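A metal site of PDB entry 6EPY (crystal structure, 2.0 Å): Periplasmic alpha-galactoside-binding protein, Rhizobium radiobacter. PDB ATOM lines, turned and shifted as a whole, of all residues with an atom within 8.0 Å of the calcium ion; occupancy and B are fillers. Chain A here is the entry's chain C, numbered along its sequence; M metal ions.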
ATOM      1  N   LYS A 457      13.336  24.515  14.536  1.00  0.00           N
ATOM      2  CA  LYS A 457      12.098  24.989  15.174  1.00  0.00           C
ATOM      3  C   LYS A 457      12.354  26.071  16.204  1.00  0.00           C
ATOM      4  O   LYS A 457      13.413  26.087  16.836  1.00  0.00           O
ATOM      5  CB  LYS A 457      11.241  23.827  15.746  1.00  0.00           C
ATOM      6  CG  LYS A 457      11.847  23.054  16.934  1.00  0.00           C
ATOM      7  CD  LYS A 457      10.843  22.084  17.550  1.00  0.00           C
ATOM      8  CE  LYS A 457      11.188  20.642  17.268  1.00  0.00           C
ATOM      9  NZ  LYS A 457      10.043  19.741  17.548  1.00  0.00           N
ATOM     10  N   ASP A 458      11.407  26.999  16.346  1.00  0.00           N
ATOM     11  CA  ASP A 458      11.502  28.097  17.319  1.00  0.00           C
ATOM     12  C   ASP A 458      11.067  27.588  18.693  1.00  0.00           C
ATOM     13  O   ASP A 458       9.863  27.475  18.975  1.00  0.00           O
ATOM     14  CB  ASP A 458      10.681  29.311  16.862  1.00  0.00           C
ATOM     15  CG  ASP A 458      10.668  30.505  17.797  1.00  0.00           C
ATOM     16  OD1 ASP A 458      11.604  30.628  18.628  1.00  0.00           O
ATOM     17  OD2 ASP A 458       9.756  31.340  17.673  1.00  0.00           O
ATOM     18  N   THR A 459      12.043  27.279  19.547  1.00  0.00           N
ATOM     19  CA  THR A 459      11.818  26.753  20.896  1.00  0.00           C
ATOM     20  C   THR A 459      11.451  27.841  21.923  1.00  0.00           C
ATOM     21  O   THR A 459      10.668  27.560  22.857  1.00  0.00           O
ATOM     22  CB  THR A 459      13.030  25.913  21.362  1.00  0.00           C
ATOM     23  OG1 THR A 459      14.156  26.764  21.539  1.00  0.00           O
ATOM     24  CG2 THR A 459      13.382  24.785  20.396  1.00  0.00           C
ATOM     25  N   ASP A 460      12.028  29.057  21.768  1.00  0.00           N
ATOM     26  CA  ASP A 460      11.907  30.220  22.676  1.00  0.00           C
ATOM     27  C   ASP A 460      10.772  31.205  22.355  1.00  0.00           C
ATOM     28  O   ASP A 460      10.549  32.147  23.119  1.00  0.00           O
ATOM     29  CB  ASP A 460      13.246  30.986  22.753  1.00  0.00           C
ATOM     30  CG  ASP A 460      14.487  30.115  22.736  1.00  0.00           C
ATOM     31  OD1 ASP A 460      14.650  29.293  23.669  1.00  0.00           O
ATOM     32  OD2 ASP A 460      15.295  30.264  21.788  1.00  0.00           O
ATOM     33  N   GLY A 461      10.077  31.008  21.243  1.00  0.00           N
ATOM     34  CA  GLY A 461       8.973  31.867  20.825  1.00  0.00           C
ATOM     35  C   GLY A 461       9.344  33.286  20.429  1.00  0.00           C
ATOM     36  O   GLY A 461       8.510  34.183  20.568  1.00  0.00           O
ATOM     37  N   ASP A 462      10.585  33.503  19.927  1.00  0.00           N
ATOM     38  CA  ASP A 462      11.062  34.815  19.449  1.00  0.00           C
ATOM     39  C   ASP A 462      10.868  35.022  17.932  1.00  0.00           C
ATOM     40  O   ASP A 462      11.338  36.012  17.367  1.00  0.00           O
ATOM     41  CB  ASP A 462      12.519  35.083  19.890  1.00  0.00           C
ATOM     42  CG  ASP A 462      13.623  34.287  19.208  1.00  0.00           C
ATOM     43  OD1 ASP A 462      13.310  33.326  18.461  1.00  0.00           O
ATOM     44  OD2 ASP A 462      14.814  34.596  19.441  1.00  0.00           O
ATOM     45  N   GLY A 463      10.183  34.082  17.280  1.00  0.00           N
ATOM     46  CA  GLY A 463       9.903  34.130  15.853  1.00  0.00           C
ATOM     47  C   GLY A 463      11.017  33.590  14.974  1.00  0.00           C
ATOM     48  O   GLY A 463      10.823  33.454  13.762  1.00  0.00           O
ATOM     49  N   PHE A 464      12.197  33.299  15.567  1.00  0.00           N
ATOM     50  CA  PHE A 464      13.354  32.773  14.840  1.00  0.00           C
ATOM     51  C   PHE A 464      13.605  31.313  15.140  1.00  0.00           C
ATOM     52  O   PHE A 464      13.485  30.895  16.285  1.00  0.00           O
ATOM     53  CB  PHE A 464      14.612  33.621  15.093  1.00  0.00           C
ATOM     54  CG  PHE A 464      14.531  34.991  14.482  1.00  0.00           C
ATOM     55  CD1 PHE A 464      14.663  35.165  13.094  1.00  0.00           C
ATOM     56  CD2 PHE A 464      14.305  36.118  15.264  1.00  0.00           C
ATOM     57  CE1 PHE A 464      14.564  36.438  12.525  1.00  0.00           C
ATOM     58  CE2 PHE A 464      14.218  37.386  14.698  1.00  0.00           C
ATOM     59  CZ  PHE A 464      14.348  37.542  13.324  1.00  0.00           C
ATOM     60  N   LEU A 465      13.972  30.529  14.126  1.00  0.00           N
ATOM     61  CA  LEU A 465      14.232  29.108  14.277  1.00  0.00           C
ATOM     62  C   LEU A 465      15.566  28.811  14.947  1.00  0.00           C
ATOM     63  O   LEU A 465      16.562  29.468  14.664  1.00  0.00           O
ATOM     64  CB  LEU A 465      14.131  28.377  12.929  1.00  0.00           C
ATOM     65  CG  LEU A 465      12.846  28.582  12.108  1.00  0.00           C
ATOM     66  CD1 LEU A 465      13.067  28.167  10.682  1.00  0.00           C
ATOM     67  CD2 LEU A 465      11.678  27.820  12.692  1.00  0.00           C
ATOM     68  N   ASN A 466      15.566  27.805  15.842  1.00  0.00           N
ATOM     69  CA  ASN A 466      16.733  27.325  16.565  1.00  0.00           C
ATOM     70  C   ASN A 466      17.237  26.022  15.929  1.00  0.00           C
ATOM     71  O   ASN A 466      16.444  25.231  15.416  1.00  0.00           O
ATOM     72  CB  ASN A 466      16.388  27.028  18.041  1.00  0.00           C
ATOM     73  CG  ASN A 466      15.923  28.221  18.826  1.00  0.00           C
ATOM     74  OD1 ASN A 466      14.873  28.806  18.559  1.00  0.00           O
ATOM     75  ND2 ASN A 466      16.706  28.595  19.835  1.00  0.00           N
ATOM     76  N   PHE A 467      18.554  25.785  16.034  1.00  0.00           N
ATOM     77  CA  PHE A 467      19.201  24.551  15.597  1.00  0.00           C
ATOM     78  C   PHE A 467      18.759  23.426  16.567  1.00  0.00           C
ATOM     79  O   PHE A 467      18.445  23.741  17.723  1.00  0.00           O
ATOM     80  CB  PHE A 467      20.733  24.695  15.741  1.00  0.00           C
ATOM     81  CG  PHE A 467      21.437  25.397  14.616  1.00  0.00           C
ATOM     82  CD1 PHE A 467      21.644  24.759  13.399  1.00  0.00           C
ATOM     83  CD2 PHE A 467      21.966  26.670  14.797  1.00  0.00           C
ATOM     84  CE1 PHE A 467      22.323  25.407  12.360  1.00  0.00           C
ATOM     85  CE2 PHE A 467      22.657  27.306  13.753  1.00  0.00           C
ATOM     86  CZ  PHE A 467      22.827  26.666  12.555  1.00  0.00           C
ATOM     87  N   GLY A 474      21.618  24.278  20.694  1.00  0.00           N
ATOM     88  CA  GLY A 474      20.267  24.721  20.387  1.00  0.00           C
ATOM     89  C   GLY A 474      20.104  26.219  20.226  1.00  0.00           C
ATOM     90  O   GLY A 474      19.017  26.745  20.453  1.00  0.00           O
ATOM     91  N   ARG A 475      21.182  26.916  19.822  1.00  0.00           N
ATOM     92  CA  ARG A 475      21.173  28.361  19.568  1.00  0.00           C
ATOM     93  C   ARG A 475      20.298  28.684  18.354  1.00  0.00           C
ATOM     94  O   ARG A 475      20.073  27.805  17.504  1.00  0.00           O
ATOM     95  CB  ARG A 475      22.605  28.847  19.253  1.00  0.00           C
ATOM     96  CG  ARG A 475      23.458  29.164  20.480  1.00  0.00           C
ATOM     97  CD  ARG A 475      24.837  29.609  20.036  1.00  0.00           C
ATOM     98  NE  ARG A 475      25.898  28.963  20.816  1.00  0.00           N
ATOM     99  CZ  ARG A 475      27.197  29.009  20.513  1.00  0.00           C
ATOM    100  NH1 ARG A 475      27.605  29.665  19.436  1.00  0.00           N
ATOM    101  NH2 ARG A 475      28.086  28.393  21.277  1.00  0.00           N
ATOM    102  N   ASN A 476      19.841  29.940  18.245  1.00  0.00           N
ATOM    103  CA  ASN A 476      19.077  30.406  17.081  1.00  0.00           C
ATOM    104  C   ASN A 476      19.983  30.334  15.835  1.00  0.00           C
ATOM    105  O   ASN A 476      21.194  30.571  15.944  1.00  0.00           O
ATOM    106  CB  ASN A 476      18.625  31.865  17.273  1.00  0.00           C
ATOM    107  CG  ASN A 476      17.316  32.066  17.999  1.00  0.00           C
ATOM    108  OD1 ASN A 476      16.465  31.173  18.093  1.00  0.00           O
ATOM    109  ND2 ASN A 476      17.099  33.268  18.486  1.00  0.00           N
ATOM    110  N   VAL A 477      19.403  29.970  14.663  1.00  0.00           N
ATOM    111  CA  VAL A 477      20.129  29.905  13.394  1.00  0.00           C
ATOM    112  C   VAL A 477      20.502  31.338  13.050  1.00  0.00           C
ATOM    113  O   VAL A 477      19.653  32.225  13.097  1.00  0.00           O
ATOM    114  CB  VAL A 477      19.327  29.199  12.257  1.00  0.00           C
ATOM    115  CG1 VAL A 477      20.091  29.215  10.931  1.00  0.00           C
ATOM    116  CG2 VAL A 477      18.971  27.761  12.654  1.00  0.00           C
ATOM    117  N   GLY A 505      11.486  32.652   9.152  1.00  0.00           N
ATOM    118  CA  GLY A 505      11.985  32.309  10.481  1.00  0.00           C
ATOM    119  C   GLY A 505      13.498  32.265  10.599  1.00  0.00           C
ATOM    120  O   GLY A 505      14.009  31.865  11.650  1.00  0.00           O
HETATM  121 CA    CA M   1      14.253  30.840  18.590  1.00  0.00          CA
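The backbone carbonyl oxygen of Gly 474 sits at hydrogen-bond distance from the side-chain amide nitrogen of Asn 466, 3.0 Å away.
The backbone carbonyl oxygen of Lys 457 lies within hydrogen-bond range of the backbone NH of Asn 466 (2.9 Å).
OD2 of Asp 458 sits at hydrogen-bond distance from N of Gly 463 (2.8 Å).
The side-chain amide nitrogen of Asn 466 is in hydrogen-bond range of the side-chain carboxylate of Asp 460 (2.9 Å).
OG1 of Thr 459 is in hydrogen-bond range of OD1 of Asp 460 (3.3 Å).
The backbone NH of Gly 461 sits close to the side-chain carboxylate of Asp 458 (3.1 Å).
The backbone NH (N) of Thr 459 lies close to the side-chain amide oxygen (OD1) of Asn 466.
Asp 460 touches the calcium ion (OD2 to CA, 3.4 Å).
Of the 16 residues printed, 6 come within 4 Å of the calcium ion.
The calcium ion is bound by the side-chain amide oxygen (OD1) of Asn 466, 2.1 Å away.
The side-chain amide oxygen (OD1) of Asn 476 is bound to the calcium ion, 2.3 Å away.
The backbone carbonyl oxygen (O) of Phe 464 binds the calcium ion.
The calcium ion is bound by the side-chain carboxylate (OD1) of Asp 458 (2.7 Å).
The calcium ion is bound by OD1 of Asp 462 (2.7 Å).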
